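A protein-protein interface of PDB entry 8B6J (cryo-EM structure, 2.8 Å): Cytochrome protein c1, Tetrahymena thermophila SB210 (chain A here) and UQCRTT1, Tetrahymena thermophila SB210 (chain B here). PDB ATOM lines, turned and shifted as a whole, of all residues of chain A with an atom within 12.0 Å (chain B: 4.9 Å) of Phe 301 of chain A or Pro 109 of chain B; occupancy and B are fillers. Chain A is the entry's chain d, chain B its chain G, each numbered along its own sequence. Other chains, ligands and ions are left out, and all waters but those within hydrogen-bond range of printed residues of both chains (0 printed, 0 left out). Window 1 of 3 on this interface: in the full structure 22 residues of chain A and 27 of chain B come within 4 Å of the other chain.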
ATOM      1  N   MET A 289       5.601  24.931   8.848  1.00  0.00           N
ATOM      2  CA  MET A 289       4.472  24.345   8.137  1.00  0.00           C
ATOM      3  C   MET A 289       3.693  25.463   7.460  1.00  0.00           C
ATOM      4  O   MET A 289       3.262  26.412   8.123  1.00  0.00           O
ATOM      5  CB  MET A 289       3.573  23.559   9.091  1.00  0.00           C
ATOM      6  CG  MET A 289       4.209  22.284   9.621  1.00  0.00           C
ATOM      7  SD  MET A 289       3.198  21.439  10.852  1.00  0.00           S
ATOM      8  CE  MET A 289       1.755  21.016   9.882  1.00  0.00           C
ATOM      9  N   TYR A 290       3.513  25.346   6.149  1.00  0.00           N
ATOM     10  CA  TYR A 290       2.873  26.371   5.340  1.00  0.00           C
ATOM     11  C   TYR A 290       1.545  25.868   4.793  1.00  0.00           C
ATOM     12  O   TYR A 290       1.220  24.680   4.860  1.00  0.00           O
ATOM     13  CB  TYR A 290       3.788  26.797   4.189  1.00  0.00           C
ATOM     14  CG  TYR A 290       5.121  27.333   4.643  1.00  0.00           C
ATOM     15  CD1 TYR A 290       5.263  28.658   5.022  1.00  0.00           C
ATOM     16  CD2 TYR A 290       6.238  26.516   4.691  1.00  0.00           C
ATOM     17  CE1 TYR A 290       6.478  29.153   5.437  1.00  0.00           C
ATOM     18  CE2 TYR A 290       7.458  27.002   5.104  1.00  0.00           C
ATOM     19  CZ  TYR A 290       7.573  28.321   5.475  1.00  0.00           C
ATOM     20  OH  TYR A 290       8.789  28.810   5.887  1.00  0.00           O
ATOM     21  N   VAL A 292      -0.361  25.063   1.697  1.00  0.00           N
ATOM     22  CA  VAL A 292      -0.254  24.721   0.284  1.00  0.00           C
ATOM     23  C   VAL A 292      -1.667  24.429  -0.202  1.00  0.00           C
ATOM     24  O   VAL A 292      -2.227  23.365   0.072  1.00  0.00           O
ATOM     25  CB  VAL A 292       0.693  23.541   0.043  1.00  0.00           C
ATOM     26  CG1 VAL A 292       2.135  23.992   0.149  1.00  0.00           C
ATOM     27  CG2 VAL A 292       0.425  22.411   1.025  1.00  0.00           C
ATOM     28  N   ASP A 294      -2.628  24.659  -3.568  1.00  0.00           N
ATOM     29  CA  ASP A 294      -2.673  24.404  -4.997  1.00  0.00           C
ATOM     30  C   ASP A 294      -3.649  23.268  -5.294  1.00  0.00           C
ATOM     31  O   ASP A 294      -3.992  22.462  -4.424  1.00  0.00           O
ATOM     32  CB  ASP A 294      -1.279  24.067  -5.529  1.00  0.00           C
ATOM     33  CG  ASP A 294      -0.611  22.947  -4.755  1.00  0.00           C
ATOM     34  OD1 ASP A 294      -1.278  22.332  -3.898  1.00  0.00           O
ATOM     35  OD2 ASP A 294       0.585  22.686  -5.000  1.00  0.00           O
ATOM     36  N   VAL A 296      -3.334  20.556  -6.646  1.00  0.00           N
ATOM     37  CA  VAL A 296      -2.823  19.194  -6.588  1.00  0.00           C
ATOM     38  C   VAL A 296      -3.453  18.445  -5.423  1.00  0.00           C
ATOM     39  O   VAL A 296      -3.576  18.968  -4.308  1.00  0.00           O
ATOM     40  CB  VAL A 296      -1.290  19.203  -6.475  1.00  0.00           C
ATOM     41  CG1 VAL A 296      -0.760  17.785  -6.342  1.00  0.00           C
ATOM     42  CG2 VAL A 296      -0.675  19.895  -7.679  1.00  0.00           C
ATOM     43  N   TYR A 297      -3.860  17.208  -5.685  1.00  0.00           N
ATOM     44  CA  TYR A 297      -4.422  16.329  -4.673  1.00  0.00           C
ATOM     45  C   TYR A 297      -3.316  15.492  -4.036  1.00  0.00           C
ATOM     46  O   TYR A 297      -2.239  15.305  -4.604  1.00  0.00           O
ATOM     47  CB  TYR A 297      -5.487  15.424  -5.296  1.00  0.00           C
ATOM     48  CG  TYR A 297      -6.333  14.664  -4.301  1.00  0.00           C
ATOM     49  CD1 TYR A 297      -7.399  15.274  -3.656  1.00  0.00           C
ATOM     50  CD2 TYR A 297      -6.078  13.331  -4.019  1.00  0.00           C
ATOM     51  CE1 TYR A 297      -8.178  14.582  -2.750  1.00  0.00           C
ATOM     52  CE2 TYR A 297      -6.851  12.631  -3.115  1.00  0.00           C
ATOM     53  CZ  TYR A 297      -7.900  13.261  -2.485  1.00  0.00           C
ATOM     54  OH  TYR A 297      -8.674  12.567  -1.584  1.00  0.00           O
ATOM     55  N   TYR A 298      -3.596  14.988  -2.835  1.00  0.00           N
ATOM     56  CA  TYR A 298      -2.622  14.185  -2.090  1.00  0.00           C
ATOM     57  C   TYR A 298      -2.811  12.707  -2.437  1.00  0.00           C
ATOM     58  O   TYR A 298      -3.223  11.880  -1.622  1.00  0.00           O
ATOM     59  CB  TYR A 298      -2.747  14.439  -0.592  1.00  0.00           C
ATOM     60  CG  TYR A 298      -4.166  14.563  -0.091  1.00  0.00           C
ATOM     61  CD1 TYR A 298      -4.897  13.442   0.273  1.00  0.00           C
ATOM     62  CD2 TYR A 298      -4.772  15.805   0.019  1.00  0.00           C
ATOM     63  CE1 TYR A 298      -6.193  13.556   0.728  1.00  0.00           C
ATOM     64  CE2 TYR A 298      -6.066  15.927   0.472  1.00  0.00           C
ATOM     65  CZ  TYR A 298      -6.771  14.802   0.828  1.00  0.00           C
ATOM     66  OH  TYR A 298      -8.062  14.923   1.278  1.00  0.00           O
ATOM     67  N   ASN A 299      -2.490  12.388  -3.692  1.00  0.00           N
ATOM     68  CA  ASN A 299      -2.635  11.018  -4.171  1.00  0.00           C
ATOM     69  C   ASN A 299      -1.647  10.080  -3.492  1.00  0.00           C
ATOM     70  O   ASN A 299      -1.976   8.921  -3.214  1.00  0.00           O
ATOM     71  CB  ASN A 299      -2.452  10.974  -5.687  1.00  0.00           C
ATOM     72  CG  ASN A 299      -3.531  11.735  -6.426  1.00  0.00           C
ATOM     73  OD1 ASN A 299      -3.245  12.657  -7.189  1.00  0.00           O
ATOM     74  ND2 ASN A 299      -4.782  11.352  -6.204  1.00  0.00           N
ATOM     75  N   HIS A 300      -0.428  10.555  -3.225  1.00  0.00           N
ATOM     76  CA  HIS A 300       0.591   9.681  -2.652  1.00  0.00           C
ATOM     77  C   HIS A 300       0.180   9.177  -1.276  1.00  0.00           C
ATOM     78  O   HIS A 300       0.402   8.007  -0.946  1.00  0.00           O
ATOM     79  CB  HIS A 300       1.929  10.412  -2.584  1.00  0.00           C
ATOM     80  CG  HIS A 300       2.594  10.564  -3.915  1.00  0.00           C
ATOM     81  ND1 HIS A 300       2.080  11.357  -4.917  1.00  0.00           N
ATOM     82  CD2 HIS A 300       3.724  10.012  -4.415  1.00  0.00           C
ATOM     83  CE1 HIS A 300       2.868  11.293  -5.975  1.00  0.00           C
ATOM     84  NE2 HIS A 300       3.873  10.483  -5.696  1.00  0.00           N
ATOM     85  N   PHE A 301      -0.411  10.044  -0.453  1.00  0.00           N
ATOM     86  CA  PHE A 301      -0.923   9.586   0.833  1.00  0.00           C
ATOM     87  C   PHE A 301      -2.045   8.573   0.643  1.00  0.00           C
ATOM     88  O   PHE A 301      -2.084   7.542   1.324  1.00  0.00           O
ATOM     89  CB  PHE A 301      -1.412  10.778   1.654  1.00  0.00           C
ATOM     90  CG  PHE A 301      -1.875  10.411   3.035  1.00  0.00           C
ATOM     91  CD1 PHE A 301      -0.962  10.063   4.014  1.00  0.00           C
ATOM     92  CD2 PHE A 301      -3.221  10.421   3.355  1.00  0.00           C
ATOM     93  CE1 PHE A 301      -1.384   9.726   5.284  1.00  0.00           C
ATOM     94  CE2 PHE A 301      -3.647  10.086   4.623  1.00  0.00           C
ATOM     95  CZ  PHE A 301      -2.727   9.739   5.588  1.00  0.00           C
ATOM     96  N   LYS A 302      -2.960   8.847  -0.287  1.00  0.00           N
ATOM     97  CA  LYS A 302      -4.101   7.962  -0.489  1.00  0.00           C
ATOM     98  C   LYS A 302      -3.680   6.652  -1.143  1.00  0.00           C
ATOM     99  O   LYS A 302      -4.187   5.582  -0.786  1.00  0.00           O
ATOM    100  CB  LYS A 302      -5.158   8.673  -1.333  1.00  0.00           C
ATOM    101  CG  LYS A 302      -6.535   8.049  -1.275  1.00  0.00           C
ATOM    102  CD  LYS A 302      -7.547   8.907  -2.013  1.00  0.00           C
ATOM    103  CE  LYS A 302      -8.949   8.338  -1.909  1.00  0.00           C
ATOM    104  NZ  LYS A 302      -9.947   9.199  -2.601  1.00  0.00           N
ATOM    105  N   TYR A 303      -2.758   6.712  -2.101  1.00  0.00           N
ATOM    106  CA  TYR A 303      -2.264   5.539  -2.819  1.00  0.00           C
ATOM    107  C   TYR A 303      -0.746   5.519  -2.679  1.00  0.00           C
ATOM    108  O   TYR A 303      -0.030   6.052  -3.530  1.00  0.00           O
ATOM    109  CB  TYR A 303      -2.676   5.567  -4.291  1.00  0.00           C
ATOM    110  CG  TYR A 303      -4.089   6.037  -4.542  1.00  0.00           C
ATOM    111  CD1 TYR A 303      -5.155   5.153  -4.493  1.00  0.00           C
ATOM    112  CD2 TYR A 303      -4.352   7.365  -4.844  1.00  0.00           C
ATOM    113  CE1 TYR A 303      -6.447   5.581  -4.728  1.00  0.00           C
ATOM    114  CE2 TYR A 303      -5.638   7.801  -5.080  1.00  0.00           C
ATOM    115  CZ  TYR A 303      -6.682   6.906  -5.021  1.00  0.00           C
ATOM    116  OH  TYR A 303      -7.965   7.340  -5.256  1.00  0.00           O
ATOM    117  N   GLY A 304      -0.253   4.902  -1.613  1.00  0.00           N
ATOM    118  CA  GLY A 304       1.181   4.837  -1.407  1.00  0.00           C
ATOM    119  C   GLY A 304       1.507   4.078  -0.143  1.00  0.00           C
ATOM    120  O   GLY A 304       0.620   3.611   0.580  1.00  0.00           O
ATOM    121  N   GLY A 305       2.799   3.959   0.110  1.00  0.00           N
ATOM    122  CA  GLY A 305       3.276   3.287   1.308  1.00  0.00           C
ATOM    123  C   GLY A 305       3.587   1.825   1.066  1.00  0.00           C
ATOM    124  O   GLY A 305       3.005   1.163   0.210  1.00  0.00           O
ATOM    125  N   TYR A 306       4.535   1.314   1.848  1.00  0.00           N
ATOM    126  CA  TYR A 306       4.941  -0.080   1.769  1.00  0.00           C
ATOM    127  C   TYR A 306       5.203  -0.597   3.174  1.00  0.00           C
ATOM    128  O   TYR A 306       5.458   0.173   4.102  1.00  0.00           O
ATOM    129  CB  TYR A 306       6.190  -0.258   0.896  1.00  0.00           C
ATOM    130  CG  TYR A 306       6.021   0.240  -0.520  1.00  0.00           C
ATOM    131  CD1 TYR A 306       5.229  -0.449  -1.427  1.00  0.00           C
ATOM    132  CD2 TYR A 306       6.657   1.396  -0.952  1.00  0.00           C
ATOM    133  CE1 TYR A 306       5.070   0.002  -2.723  1.00  0.00           C
ATOM    134  CE2 TYR A 306       6.506   1.854  -2.245  1.00  0.00           C
ATOM    135  CZ  TYR A 306       5.712   1.152  -3.127  1.00  0.00           C
ATOM    136  OH  TYR A 306       5.559   1.603  -4.417  1.00  0.00           O
ATOM    137  N   ALA B 103      -6.543   5.044   7.549  1.00  0.00           N
ATOM    138  CA  ALA B 103      -6.260   6.471   7.467  1.00  0.00           C
ATOM    139  C   ALA B 103      -5.948   6.890   6.039  1.00  0.00           C
ATOM    140  O   ALA B 103      -6.429   7.928   5.570  1.00  0.00           O
ATOM    141  CB  ALA B 103      -5.097   6.824   8.392  1.00  0.00           C
ATOM    142  N   ARG B 104      -5.144   6.099   5.327  1.00  0.00           N
ATOM    143  CA  ARG B 104      -4.818   6.440   3.949  1.00  0.00           C
ATOM    144  C   ARG B 104      -6.064   6.447   3.077  1.00  0.00           C
ATOM    145  O   ARG B 104      -6.243   7.342   2.244  1.00  0.00           O
ATOM    146  CB  ARG B 104      -3.785   5.462   3.393  1.00  0.00           C
ATOM    147  CG  ARG B 104      -2.385   5.652   3.946  1.00  0.00           C
ATOM    148  CD  ARG B 104      -1.397   4.726   3.261  1.00  0.00           C
ATOM    149  NE  ARG B 104      -0.030   4.940   3.719  1.00  0.00           N
ATOM    150  CZ  ARG B 104       0.791   5.861   3.234  1.00  0.00           C
ATOM    151  NH1 ARG B 104       0.412   6.693   2.277  1.00  0.00           N
ATOM    152  NH2 ARG B 104       2.025   5.953   3.722  1.00  0.00           N
ATOM    153  N   LEU B 107      -8.951   9.011   5.877  1.00  0.00           N
ATOM    154  CA  LEU B 107      -8.614  10.224   6.605  1.00  0.00           C
ATOM    155  C   LEU B 107      -7.844  11.212   5.737  1.00  0.00           C
ATOM    156  O   LEU B 107      -7.160  10.841   4.779  1.00  0.00           O
ATOM    157  CB  LEU B 107      -7.789   9.893   7.846  1.00  0.00           C
ATOM    158  CG  LEU B 107      -8.532   9.265   9.025  1.00  0.00           C
ATOM    159  CD1 LEU B 107      -7.559   8.985  10.157  1.00  0.00           C
ATOM    160  CD2 LEU B 107      -9.665  10.160   9.502  1.00  0.00           C
ATOM    161  N   HIS B 108      -7.977  12.490   6.085  1.00  0.00           N
ATOM    162  CA  HIS B 108      -7.178  13.570   5.536  1.00  0.00           C
ATOM    163  C   HIS B 108      -5.789  13.561   6.175  1.00  0.00           C
ATOM    164  O   HIS B 108      -5.637  13.160   7.331  1.00  0.00           O
ATOM    165  CB  HIS B 108      -7.867  14.905   5.798  1.00  0.00           C
ATOM    166  CG  HIS B 108      -7.337  16.041   4.982  1.00  0.00           C
ATOM    167  ND1 HIS B 108      -6.304  16.845   5.408  1.00  0.00           N
ATOM    168  CD2 HIS B 108      -7.711  16.520   3.772  1.00  0.00           C
ATOM    169  CE1 HIS B 108      -6.055  17.763   4.493  1.00  0.00           C
ATOM    170  NE2 HIS B 108      -6.896  17.588   3.490  1.00  0.00           N
ATOM    171  N   PRO B 109      -4.752  13.989   5.448  1.00  0.00           N
ATOM    172  CA  PRO B 109      -3.405  13.969   6.044  1.00  0.00           C
ATOM    173  C   PRO B 109      -3.292  14.762   7.333  1.00  0.00           C
ATOM    174  O   PRO B 109      -2.525  14.370   8.221  1.00  0.00           O
ATOM    175  CB  PRO B 109      -2.529  14.568   4.937  1.00  0.00           C
ATOM    176  CG  PRO B 109      -3.245  14.255   3.686  1.00  0.00           C
ATOM    177  CD  PRO B 109      -4.706  14.328   4.015  1.00  0.00           C
ATOM    178  N   TYR B 110      -4.033  15.865   7.470  1.00  0.00           N
ATOM    179  CA  TYR B 110      -3.885  16.717   8.647  1.00  0.00           C
ATOM    180  C   TYR B 110      -4.276  15.985   9.925  1.00  0.00           C
ATOM    181  O   TYR B 110      -3.637  16.165  10.968  1.00  0.00           O
ATOM    182  CB  TYR B 110      -4.722  17.988   8.486  1.00  0.00           C
ATOM    183  CG  TYR B 110      -4.008  19.151   7.819  1.00  0.00           C
ATOM    184  CD1 TYR B 110      -2.769  18.992   7.215  1.00  0.00           C
ATOM    185  CD2 TYR B 110      -4.578  20.416   7.809  1.00  0.00           C
ATOM    186  CE1 TYR B 110      -2.125  20.052   6.618  1.00  0.00           C
ATOM    187  CE2 TYR B 110      -3.937  21.482   7.213  1.00  0.00           C
ATOM    188  CZ  TYR B 110      -2.713  21.294   6.620  1.00  0.00           C
ATOM    189  OH  TYR B 110      -2.071  22.354   6.024  1.00  0.00           O
ATOM    190  N   THR B 111      -5.322  15.158   9.868  1.00  0.00           N
ATOM    191  CA  THR B 111      -5.831  14.526  11.081  1.00  0.00           C
ATOM    192  C   THR B 111      -4.731  13.789  11.836  1.00  0.00           C
ATOM    193  O   THR B 111      -4.732  13.756  13.072  1.00  0.00           O
ATOM    194  CB  THR B 111      -6.964  13.561  10.737  1.00  0.00           C
ATOM    195  OG1 THR B 111      -6.466  12.520   9.890  1.00  0.00           O
ATOM    196  CG2 THR B 111      -8.088  14.287  10.028  1.00  0.00           C
ATOM    197  N   VAL B 112      -3.786  13.190  11.114  1.00  0.00           N
ATOM    198  CA  VAL B 112      -2.709  12.430  11.736  1.00  0.00           C
ATOM    199  C   VAL B 112      -1.451  13.288  11.799  1.00  0.00           C
ATOM    200  O   VAL B 112      -0.616  13.126  12.699  1.00  0.00           O
ATOM    201  CB  VAL B 112      -2.451  11.116  10.975  1.00  0.00           C
ATOM    202  CG1 VAL B 112      -1.910  11.396   9.580  1.00  0.00           C
ATOM    203  CG2 VAL B 112      -1.500  10.226  11.758  1.00  0.00           C
ATOM    204  N   LEU B 113      -1.306  14.208  10.843  1.00  0.00           N
ATOM    205  CA  LEU B 113      -0.132  15.073  10.822  1.00  0.00           C
ATOM    206  C   LEU B 113      -0.058  15.923  12.084  1.00  0.00           C
ATOM    207  O   LEU B 113       1.003  16.036  12.707  1.00  0.00           O
ATOM    208  CB  LEU B 113      -0.165  15.959   9.577  1.00  0.00           C
ATOM    209  CG  LEU B 113       0.995  16.940   9.406  1.00  0.00           C
ATOM    210  CD1 LEU B 113       2.308  16.198   9.236  1.00  0.00           C
ATOM    211  CD2 LEU B 113       0.737  17.859   8.227  1.00  0.00           C
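The backbone carbonyl oxygen (O) of His 300 of chain A sits at hydrogen-bond distance from the guanidinium group (NH1) of Arg 104 of chain B.
O of Phe 301 of chain A sits at hydrogen-bond distance from NH1 of Arg 104 of chain B (2.8 Å).
The backbone carbonyl oxygen (O) of Gly 304 of chain A lies within hydrogen-bond range of the guanidinium group (NE) of Arg 104 of chain B, 3.5 Å away.
The backbone NH (N) of Tyr 110 of chain B sits close to a ring nitrogen (ND1) of His 108 of chain B (3.2 Å).
O of His 108 of chain B is in hydrogen-bond range of OG1 of Thr 111 of chain B (2.8 Å).
CE of Met 289 of chain A touches CD2 of Leu 113 of chain B, 3.7 Å away.
Tyr 298 of chain A touches His 108 of chain B (OH to CD2, 3.0 Å).
CE1 of Tyr 298 of chain A touches CD of Pro 109 of chain B (3.7 Å).
Phe 301 of chain A touches Ala 103 of chain B.
Phe 301 of chain A touches Leu 107 of chain B (CE2 to O, 3.6 Å).
CG of Pro 109 of chain B touches CD2 of Phe 301 of chain A (3.8 Å).
Arg 104 of chain B touches Lys 302 of chain A (O to CA, 3.5 Å).
Arg 104 of chain B touches Gly 305 of chain A (NH2 to CA, 3.8 Å).
Of chain B, only Ala 103, Arg 104, Leu 107 and Pro 109 come within 4 Å of Phe 301 of chain A.
Printed residues of chain B within 4 Å of Lys 302 of chain A: Arg 104.
Of the printed residues of chain B, Gly 304 of chain A touches Arg 104 (3.5 Å).
Of chain A, only His 300, Phe 301, Lys 302, Gly 304 and Gly 305 come within 4 Å of Arg 104 of chain B.
Of chain A, only Tyr 298 comes within 4 Å of His 108 of chain B.
Of chain A, only Tyr 298 (3.7 Å) and Phe 301 (3.8 Å) come within 4 Å of Pro 109 of chain B.
No residue of chain A comes within 4 Å of Tyr 110 of chain B.
No residue of chain A comes within 4 Å of Thr 111 of chain B.
Leu 113 of chain B touches one residue of chain A.
The nearest residue of chain B that does not touch Phe 301 of chain A is His 108 of chain B (4.4 Å).
The nearest residue of chain A that does not touch Pro 109 of chain B is Lys 302 of chain A (6.7 Å).
Hydrophobic or aromatic side chains of chain A within 4 Å of the printed part of chain B: Met 289, Tyr 298 and Phe 301.
Of the 9 printed residues of chain B, 6 touch a printed residue of chain A.
Among the printed residues, 11 pairs touch across the chains.
Among the printed residues, no Asp or Glu carboxylate lies within 4 Å of a Lys or Arg side-chain nitrogen of the other chain.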
